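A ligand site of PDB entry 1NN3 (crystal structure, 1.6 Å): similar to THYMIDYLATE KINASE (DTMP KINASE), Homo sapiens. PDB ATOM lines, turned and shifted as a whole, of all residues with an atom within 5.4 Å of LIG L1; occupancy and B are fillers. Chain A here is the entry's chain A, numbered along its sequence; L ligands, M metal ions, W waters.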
ATOM      1  N   LYS A  22       0.358  -1.039  -8.152  1.00  0.00           N
ATOM      2  CA  LYS A  22       1.017  -2.349  -8.179  1.00  0.00           C
ATOM      3  C   LYS A  22       2.464  -2.220  -8.598  1.00  0.00           C
ATOM      4  O   LYS A  22       3.358  -2.782  -7.967  1.00  0.00           O
ATOM      5  CB  LYS A  22       0.294  -3.297  -9.144  1.00  0.00           C
ATOM      6  CG  LYS A  22      -1.182  -3.507  -8.787  1.00  0.00           C
ATOM      7  CD  LYS A  22      -1.887  -4.389  -9.834  1.00  0.00           C
ATOM      8  CE  LYS A  22      -2.075  -3.664 -11.173  1.00  0.00           C
ATOM      9  NZ  LYS A  22      -2.960  -2.488 -11.021  1.00  0.00           N
ATOM     10  N   SER A  23       2.709  -1.541  -9.723  1.00  0.00           N
ATOM     11  CA  SER A  23       4.087  -1.483 -10.185  1.00  0.00           C
ATOM     12  C   SER A  23       4.976  -0.656  -9.248  1.00  0.00           C
ATOM     13  O   SER A  23       6.109  -1.065  -8.950  1.00  0.00           O
ATOM     14  CB  SER A  23       4.130  -0.973 -11.632  1.00  0.00           C
ATOM     15  OG  SER A  23       3.327  -1.857 -12.421  1.00  0.00           O
ATOM     16  N   PHE A  45       3.645  -9.843 -14.734  1.00  0.00           N
ATOM     17  CA  PHE A  45       2.883 -10.525 -15.788  1.00  0.00           C
ATOM     18  C   PHE A  45       1.927  -9.505 -16.365  1.00  0.00           C
ATOM     19  O   PHE A  45       1.328  -8.697 -15.632  1.00  0.00           O
ATOM     20  CB  PHE A  45       2.172 -11.773 -15.228  1.00  0.00           C
ATOM     21  CG  PHE A  45       3.190 -12.848 -14.908  1.00  0.00           C
ATOM     22  CD1 PHE A  45       3.551 -13.105 -13.604  1.00  0.00           C
ATOM     23  CD2 PHE A  45       3.800 -13.536 -15.948  1.00  0.00           C
ATOM     24  CE1 PHE A  45       4.495 -14.070 -13.304  1.00  0.00           C
ATOM     25  CE2 PHE A  45       4.743 -14.502 -15.638  1.00  0.00           C
ATOM     26  CZ  PHE A  45       5.111 -14.791 -14.328  1.00  0.00           C
ATOM     27  N   PRO A  46       1.760  -9.480 -17.690  1.00  0.00           N
ATOM     28  CA  PRO A  46       2.500 -10.340 -18.575  1.00  0.00           C
ATOM     29  C   PRO A  46       3.971  -9.998 -18.654  1.00  0.00           C
ATOM     30  O   PRO A  46       4.390  -8.839 -18.440  1.00  0.00           O
ATOM     31  CB  PRO A  46       1.858 -10.067 -19.948  1.00  0.00           C
ATOM     32  CG  PRO A  46       1.367  -8.645 -19.820  1.00  0.00           C
ATOM     33  CD  PRO A  46       0.882  -8.528 -18.392  1.00  0.00           C
ATOM     34  N   ARG A  48       6.401  -9.441 -21.007  1.00  0.00           N
ATOM     35  CA  ARG A  48       6.315  -9.114 -22.432  1.00  0.00           C
ATOM     36  C   ARG A  48       7.525  -9.457 -23.253  1.00  0.00           C
ATOM     37  O   ARG A  48       7.463  -9.228 -24.487  1.00  0.00           O
ATOM     38  CB  ARG A  48       5.957  -7.610 -22.560  1.00  0.00           C
ATOM     39  CG  ARG A  48       4.592  -7.302 -21.941  1.00  0.00           C
ATOM     40  CD  ARG A  48       4.257  -5.820 -22.061  1.00  0.00           C
ATOM     41  NE  ARG A  48       3.178  -5.394 -21.173  1.00  0.00           N
ATOM     42  CZ  ARG A  48       2.186  -4.618 -21.620  1.00  0.00           C
ATOM     43  NH1 ARG A  48       2.127  -4.209 -22.883  1.00  0.00           N
ATOM     44  NH2 ARG A  48       1.219  -4.211 -20.812  1.00  0.00           N
ATOM     45  N   LEU A  60      -2.514  -5.982 -26.259  1.00  0.00           N
ATOM     46  CA  LEU A  60      -2.878  -4.943 -25.286  1.00  0.00           C
ATOM     47  C   LEU A  60      -2.721  -3.550 -25.912  1.00  0.00           C
ATOM     48  O   LEU A  60      -3.465  -2.640 -25.545  1.00  0.00           O
ATOM     49  CB  LEU A  60      -2.018  -5.053 -24.014  1.00  0.00           C
ATOM     50  CG  LEU A  60      -2.317  -6.285 -23.163  1.00  0.00           C
ATOM     51  CD1 LEU A  60      -1.290  -6.432 -22.050  1.00  0.00           C
ATOM     52  CD2 LEU A  60      -3.716  -6.193 -22.572  1.00  0.00           C
ATOM     53  N   PHE A  75      -2.095 -15.656 -22.052  1.00  0.00           N
ATOM     54  CA  PHE A  75      -1.694 -15.036 -20.768  1.00  0.00           C
ATOM     55  C   PHE A  75      -1.286 -16.100 -19.745  1.00  0.00           C
ATOM     56  O   PHE A  75      -0.335 -15.906 -18.986  1.00  0.00           O
ATOM     57  CB  PHE A  75      -2.826 -14.176 -20.211  1.00  0.00           C
ATOM     58  CG  PHE A  75      -2.902 -12.748 -20.701  1.00  0.00           C
ATOM     59  CD1 PHE A  75      -3.969 -12.355 -21.491  1.00  0.00           C
ATOM     60  CD2 PHE A  75      -1.932 -11.852 -20.317  1.00  0.00           C
ATOM     61  CE1 PHE A  75      -4.042 -11.024 -21.922  1.00  0.00           C
ATOM     62  CE2 PHE A  75      -2.010 -10.515 -20.727  1.00  0.00           C
ATOM     63  CZ  PHE A  75      -3.064 -10.126 -21.517  1.00  0.00           C
ATOM     64  N   SER A  76      -2.016 -17.212 -19.713  1.00  0.00           N
ATOM     65  CA  SER A  76      -1.685 -18.292 -18.746  1.00  0.00           C
ATOM     66  C   SER A  76      -0.393 -18.956 -19.160  1.00  0.00           C
ATOM     67  O   SER A  76       0.480 -19.282 -18.329  1.00  0.00           O
ATOM     68  CB  SER A  76      -2.856 -19.273 -18.665  1.00  0.00           C
ATOM     69  OG  SER A  76      -2.490 -20.335 -17.795  1.00  0.00           O
ATOM     70  N   ARG A  79       2.615 -17.312 -17.934  1.00  0.00           N
ATOM     71  CA  ARG A  79       2.993 -17.615 -16.544  1.00  0.00           C
ATOM     72  C   ARG A  79       3.659 -18.977 -16.477  1.00  0.00           C
ATOM     73  O   ARG A  79       4.728 -19.063 -15.839  1.00  0.00           O
ATOM     74  CB  ARG A  79       1.764 -17.561 -15.619  1.00  0.00           C
ATOM     75  CG  ARG A  79       1.386 -16.118 -15.261  1.00  0.00           C
ATOM     76  CD  ARG A  79       0.125 -16.109 -14.434  1.00  0.00           C
ATOM     77  NE  ARG A  79      -1.136 -16.507 -15.100  1.00  0.00           N
ATOM     78  CZ  ARG A  79      -1.824 -15.637 -15.846  1.00  0.00           C
ATOM     79  NH1 ARG A  79      -1.300 -14.427 -16.096  1.00  0.00           N
ATOM     80  NH2 ARG A  79      -2.996 -15.998 -16.362  1.00  0.00           N
ATOM     81  N   ASP A  99       4.245  -8.499  -9.900  1.00  0.00           N
ATOM     82  CA  ASP A  99       3.292  -7.461 -10.283  1.00  0.00           C
ATOM     83  C   ASP A  99       2.287  -8.086 -11.239  1.00  0.00           C
ATOM     84  O   ASP A  99       2.606  -8.243 -12.426  1.00  0.00           O
ATOM     85  CB  ASP A  99       4.122  -6.346 -10.916  1.00  0.00           C
ATOM     86  CG  ASP A  99       3.342  -5.149 -11.392  1.00  0.00           C
ATOM     87  OD1 ASP A  99       2.111  -5.104 -11.315  1.00  0.00           O
ATOM     88  OD2 ASP A  99       4.060  -4.267 -11.988  1.00  0.00           O
ATOM     89  N   ARG A 100       1.162  -8.490 -10.720  1.00  0.00           N
ATOM     90  CA  ARG A 100       0.096  -9.205 -11.388  1.00  0.00           C
ATOM     91  C   ARG A 100       0.432 -10.717 -11.534  1.00  0.00           C
ATOM     92  O   ARG A 100       1.576 -11.100 -11.778  1.00  0.00           O
ATOM     93  CB  ARG A 100      -0.334  -8.678 -12.751  1.00  0.00           C
ATOM     94  CG  ARG A 100      -0.924  -7.247 -12.717  1.00  0.00           C
ATOM     95  CD  ARG A 100      -1.557  -7.025 -14.106  1.00  0.00           C
ATOM     96  NE  ARG A 100      -1.981  -5.664 -14.356  1.00  0.00           N
ATOM     97  CZ  ARG A 100      -3.194  -5.203 -14.014  1.00  0.00           C
ATOM     98  NH1 ARG A 100      -4.136  -5.909 -13.365  1.00  0.00           N
ATOM     99  NH2 ARG A 100      -3.433  -3.917 -14.286  1.00  0.00           N
ATOM    100  N   TYR A 101      -0.655 -11.488 -11.423  1.00  0.00           N
ATOM    101  CA  TYR A 101      -0.482 -12.954 -11.600  1.00  0.00           C
ATOM    102  C   TYR A 101      -1.758 -13.546 -12.171  1.00  0.00           C
ATOM    103  O   TYR A 101      -2.460 -12.871 -12.911  1.00  0.00           O
ATOM    104  CB  TYR A 101      -0.071 -13.580 -10.281  1.00  0.00           C
ATOM    105  CG  TYR A 101       0.538 -14.965 -10.208  1.00  0.00           C
ATOM    106  CD1 TYR A 101       1.674 -15.282 -10.918  1.00  0.00           C
ATOM    107  CD2 TYR A 101       0.005 -15.915  -9.351  1.00  0.00           C
ATOM    108  CE1 TYR A 101       2.261 -16.555 -10.812  1.00  0.00           C
ATOM    109  CE2 TYR A 101       0.568 -17.195  -9.206  1.00  0.00           C
ATOM    110  CZ  TYR A 101       1.700 -17.475  -9.962  1.00  0.00           C
ATOM    111  OH  TYR A 101       2.350 -18.702  -9.828  1.00  0.00           O
ATOM    112  N   SER A 104      -5.221 -11.494 -12.003  1.00  0.00           N
ATOM    113  CA  SER A 104      -5.537 -10.555 -13.098  1.00  0.00           C
ATOM    114  C   SER A 104      -5.979 -11.332 -14.343  1.00  0.00           C
ATOM    115  O   SER A 104      -6.907 -10.933 -15.057  1.00  0.00           O
ATOM    116  CB  SER A 104      -4.328  -9.719 -13.488  1.00  0.00           C
ATOM    117  OG  SER A 104      -4.200  -8.590 -12.605  1.00  0.00           O
ATOM    118  N   GLY A 105      -5.337 -12.465 -14.611  1.00  0.00           N
ATOM    119  CA  GLY A 105      -5.746 -13.249 -15.805  1.00  0.00           C
ATOM    120  C   GLY A 105      -7.235 -13.603 -15.719  1.00  0.00           C
ATOM    121  O   GLY A 105      -7.972 -13.517 -16.726  1.00  0.00           O
ATOM    122  N   PHE A 108      -9.718 -10.187 -15.703  1.00  0.00           N
ATOM    123  CA  PHE A 108      -9.837  -9.476 -16.960  1.00  0.00           C
ATOM    124  C   PHE A 108     -10.597 -10.288 -17.980  1.00  0.00           C
ATOM    125  O   PHE A 108     -11.488  -9.720 -18.661  1.00  0.00           O
ATOM    126  CB  PHE A 108      -8.477  -8.959 -17.455  1.00  0.00           C
ATOM    127  CG  PHE A 108      -8.146  -7.701 -16.668  1.00  0.00           C
ATOM    128  CD1 PHE A 108      -7.626  -7.826 -15.391  1.00  0.00           C
ATOM    129  CD2 PHE A 108      -8.453  -6.456 -17.159  1.00  0.00           C
ATOM    130  CE1 PHE A 108      -7.372  -6.691 -14.633  1.00  0.00           C
ATOM    131  CE2 PHE A 108      -8.199  -5.322 -16.391  1.00  0.00           C
ATOM    132  CZ  PHE A 108      -7.660  -5.435 -15.133  1.00  0.00           C
ATOM    133  N   THR A 109     -10.281 -11.573 -18.189  1.00  0.00           N
ATOM    134  CA  THR A 109     -11.116 -12.308 -19.153  1.00  0.00           C
ATOM    135  C   THR A 109     -12.515 -12.525 -18.612  1.00  0.00           C
ATOM    136  O   THR A 109     -13.512 -12.503 -19.355  1.00  0.00           O
ATOM    137  CB  THR A 109     -10.471 -13.677 -19.480  1.00  0.00           C
ATOM    138  OG1 THR A 109      -9.219 -13.352 -20.095  1.00  0.00           O
ATOM    139  CG2 THR A 109     -11.361 -14.482 -20.415  1.00  0.00           C
ATOM    140  N   GLU A 152      -4.277   1.407 -23.617  1.00  0.00           N
ATOM    141  CA  GLU A 152      -4.237  -0.037 -23.857  1.00  0.00           C
ATOM    142  C   GLU A 152      -5.649  -0.597 -23.702  1.00  0.00           C
ATOM    143  O   GLU A 152      -6.571   0.002 -23.140  1.00  0.00           O
ATOM    144  CB  GLU A 152      -3.271  -0.816 -22.968  1.00  0.00           C
ATOM    145  CG  GLU A 152      -1.799  -0.735 -23.342  1.00  0.00           C
ATOM    146  CD  GLU A 152      -0.864  -1.780 -22.769  1.00  0.00           C
ATOM    147  OE1 GLU A 152      -1.100  -2.401 -21.707  1.00  0.00           O
ATOM    148  OE2 GLU A 152       0.201  -2.031 -23.393  1.00  0.00           O
ATOM    149  N   TYR A 154      -8.749  -2.598 -22.294  1.00  0.00           N
ATOM    150  CA  TYR A 154      -9.283  -2.758 -20.964  1.00  0.00           C
ATOM    151  C   TYR A 154      -9.200  -1.490 -20.096  1.00  0.00           C
ATOM    152  O   TYR A 154      -9.665  -1.530 -18.969  1.00  0.00           O
ATOM    153  CB  TYR A 154      -8.538  -3.853 -20.194  1.00  0.00           C
ATOM    154  CG  TYR A 154      -8.505  -5.198 -20.877  1.00  0.00           C
ATOM    155  CD1 TYR A 154      -7.475  -6.089 -20.584  1.00  0.00           C
ATOM    156  CD2 TYR A 154      -9.476  -5.587 -21.792  1.00  0.00           C
ATOM    157  CE1 TYR A 154      -7.412  -7.344 -21.173  1.00  0.00           C
ATOM    158  CE2 TYR A 154      -9.418  -6.833 -22.390  1.00  0.00           C
ATOM    159  CZ  TYR A 154      -8.390  -7.702 -22.084  1.00  0.00           C
ATOM    160  OH  TYR A 154      -8.337  -8.942 -22.662  1.00  0.00           O
HETATM  161  P1  LIG L   1      -0.142  -3.681 -16.846  1.00  0.00           P
HETATM  162  O1  LIG L   1       1.083  -3.915 -17.744  1.00  0.00           O
HETATM  163  O2  LIG L   1      -0.339  -2.197 -16.869  1.00  0.00           O
HETATM  164  O3  LIG L   1      -0.032  -4.480 -15.580  1.00  0.00           O
HETATM  165  O4  LIG L   1      -1.251  -4.177 -17.851  1.00  0.00           O
HETATM  166  N1  LIG L   1      -4.036  -8.849 -18.047  1.00  0.00           N
HETATM  167  C1  LIG L   1      -2.931  -9.128 -17.251  1.00  0.00           C
HETATM  168  C2  LIG L   1      -4.829  -9.856 -18.610  1.00  0.00           C
HETATM  169  O5  LIG L   1      -5.805  -9.639 -19.308  1.00  0.00           O
HETATM  170  N2  LIG L   1      -4.453 -11.148 -18.283  1.00  0.00           N
HETATM  171  C3  LIG L   1      -3.388 -11.496 -17.496  1.00  0.00           C
HETATM  172  O6  LIG L   1      -3.164 -12.702 -17.296  1.00  0.00           O
HETATM  173  C4  LIG L   1      -2.630 -10.400 -16.985  1.00  0.00           C
HETATM  174  C5  LIG L   1      -1.444 -10.756 -16.094  1.00  0.00           C
HETATM  175  C6  LIG L   1      -4.627  -6.536 -17.397  1.00  0.00           C
HETATM  176  C7  LIG L   1      -1.397  -5.582 -18.185  1.00  0.00           C
HETATM  177  C8  LIG L   1      -2.853  -5.657 -18.586  1.00  0.00           C
HETATM  178  O7  LIG L   1      -3.133  -6.994 -19.109  1.00  0.00           O
HETATM  179  C9  LIG L   1      -4.311  -7.484 -18.502  1.00  0.00           C
HETATM  180  C10 LIG L   1      -3.813  -5.521 -17.479  1.00  0.00           C
HETATM  181  P1  LG2 L   2      -0.454   0.177 -11.411  1.00  0.00           P
HETATM  182  O1  LG2 L   2      -1.316  -0.406 -10.349  1.00  0.00           O
HETATM  183  O2  LG2 L   2       0.736  -0.569 -11.840  1.00  0.00           O
HETATM  184  O3  LG2 L   2      -1.285   0.621 -12.700  1.00  0.00           O
HETATM  185  P2  LG2 L   2       1.350   2.450 -10.880  1.00  0.00           P
HETATM  186  O4  LG2 L   2       1.913   2.467 -12.247  1.00  0.00           O
HETATM  187  O5  LG2 L   2       2.291   1.999  -9.800  1.00  0.00           O
HETATM  188  O6  LG2 L   2      -0.015   1.620 -10.778  1.00  0.00           O
HETATM  189  O7  LG2 L   2       0.888   3.882 -10.447  1.00  0.00           O
HETATM  190  C1  LG2 L   2      -0.006   4.600 -11.351  1.00  0.00           C
HETATM  191  C2  LG2 L   2       0.332   6.092 -11.210  1.00  0.00           C
HETATM  192  O8  LG2 L   2      -0.139   6.536  -9.943  1.00  0.00           O
HETATM  193  C3  LG2 L   2       1.815   6.419 -11.311  1.00  0.00           C
HETATM  194  O9  LG2 L   2       1.953   7.714 -11.879  1.00  0.00           O
HETATM  195  C4  LG2 L   2       2.212   6.503  -9.821  1.00  0.00           C
HETATM  196  O10 LG2 L   2       3.305   7.334  -9.572  1.00  0.00           O
HETATM  197  C5  LG2 L   2       0.924   7.016  -9.174  1.00  0.00           C
HETATM  198  N1  LG2 L   2       0.793   6.473  -7.805  1.00  0.00           N
HETATM  199  C6  LG2 L   2       1.139   5.211  -7.375  1.00  0.00           C
HETATM  200  N2  LG2 L   2       0.857   5.008  -6.100  1.00  0.00           N
HETATM  201  C7  LG2 L   2       0.313   6.239  -5.655  1.00  0.00           C
HETATM  202  C8  LG2 L   2      -0.150   6.655  -4.421  1.00  0.00           C
HETATM  203  N3  LG2 L   2      -0.181   5.956  -3.340  1.00  0.00           N
HETATM  204  N4  LG2 L   2      -0.620   7.932  -4.451  1.00  0.00           N
HETATM  205  C9  LG2 L   2      -0.621   8.705  -5.524  1.00  0.00           C
HETATM  206  N5  LG2 L   2      -0.197   8.392  -6.746  1.00  0.00           N
HETATM  207  C10 LG2 L   2       0.257   7.139  -6.694  1.00  0.00           C
HETATM  208 MG    MG M   1       1.535  -1.390 -13.454  1.00  0.00          MG
HETATM  209  O   HOH W   1       2.551  -2.140 -15.191  1.00  0.00           O
HETATM  210  O   HOH W   2       2.228  -6.089 -15.398  1.00  0.00           O
HETATM  211  O   HOH W   3       3.409  -2.276 -18.371  1.00  0.00           O
HETATM  212  O   HOH W   4       3.543  -6.361 -17.911  1.00  0.00           O
HETATM  213  O   HOH W   5       0.119  -0.842 -18.819  1.00  0.00           O
HETATM  214  O   HOH W   6      -7.693 -10.837 -20.806  1.00  0.00           O
HETATM  215  O   HOH W   7      -0.136  -1.132 -14.579  1.00  0.00           O
HETATM  216  O   HOH W   8       0.905  -3.367 -13.042  1.00  0.00           O
HETATM  217  O   HOH W   9      -6.202 -13.274 -19.025  1.00  0.00           O
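An oxygen (O3) of LIG L1 lies within salt-bridge range of the guanidinium group (NE) of Arg 100 (2.6 Å).
NH1 of Arg 79 lies within hydrogen-bond range of O6 of LIG L1 (2.8 Å).
The backbone NH (N) of Gly 105 sits close to an oxygen (O6) of LIG L1, 3.5 Å away.
The guanidinium group of Arg 48 is in salt-bridge range of an oxygen (O1) of LIG L1.
O1 of LG2 L2 sits at hydrogen-bond distance from N of Lys 22 (2.8 Å).
NZ of Lys 22 is in salt-bridge range of O1 of LG2 L2, at 2.7 Å.
The backbone NH (N) of Ser 23 lies close to an oxygen (O2) of LG2 L2 (3.1 Å).
The side-chain hydroxyl (OG) of Ser 104 lies within hydrogen-bond range of the guanidinium group (NH1) of Arg 100 (2.8 Å).
NH1 of Arg 79 is in hydrogen-bond range of O of Phe 75 (3.4 Å).
NH1 of Arg 48 is in salt-bridge range of OE2 of Glu 152, at 3.0 Å.
N of Phe 45 is in hydrogen-bond range of O of Asp 99, at 3.0 Å.
Residues that only touch LIG L1: Phe 45, Pro 46, Leu 60, Phe 75, Tyr 101, Ser 104, Phe 108 and Tyr 154.
12 residues have an atom within 4 Å of LIG L1: Phe 45, Pro 46, Arg 48, Leu 60, Phe 75, Arg 79, Arg 100, Tyr 101, Ser 104, Gly 105, Phe 108 and Tyr 154.
Along chain A the residues within 4 Å of LIG L1 span positions 45 to 154.
The nearest printed residue that does not touch LIG L1 is Glu 152 (4.2 Å).
Water W7 bridges O2 of LIG L1 (2.5 Å) and O3 of LG2 L2 (2.8 Å).
Water W6 lies within hydrogen-bond range of an oxygen (O5) of LIG L1 (2.7 Å), the side-chain hydroxyl (OH) of Tyr 154 (2.7 Å) and the side-chain hydroxyl (OG1) of Thr 109 (3.0 Å).
Water W2 lies within hydrogen-bond range of the backbone carbonyl oxygen (O) of Phe 45 (2.8 Å) and an oxygen (O3) of LIG L1 (2.8 Å).
Water W9 lies within hydrogen-bond range of N2 of LIG L1 (2.9 Å), O of Gly 105 (2.9 Å) and OG1 of Thr 109 (3.2 Å).
Water W8 lies within hydrogen-bond range of the side-chain carboxylate of Asp 99 (2.7 Å) and an oxygen (O3) of LIG L1 (2.9 Å).
Water W4 lies within hydrogen-bond range of the backbone carbonyl oxygen (O) of Pro 46 (2.7 Å), the guanidinium group (NE) of Arg 48 (3.4 Å) and an oxygen (O1) of LIG L1 (3.5 Å).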
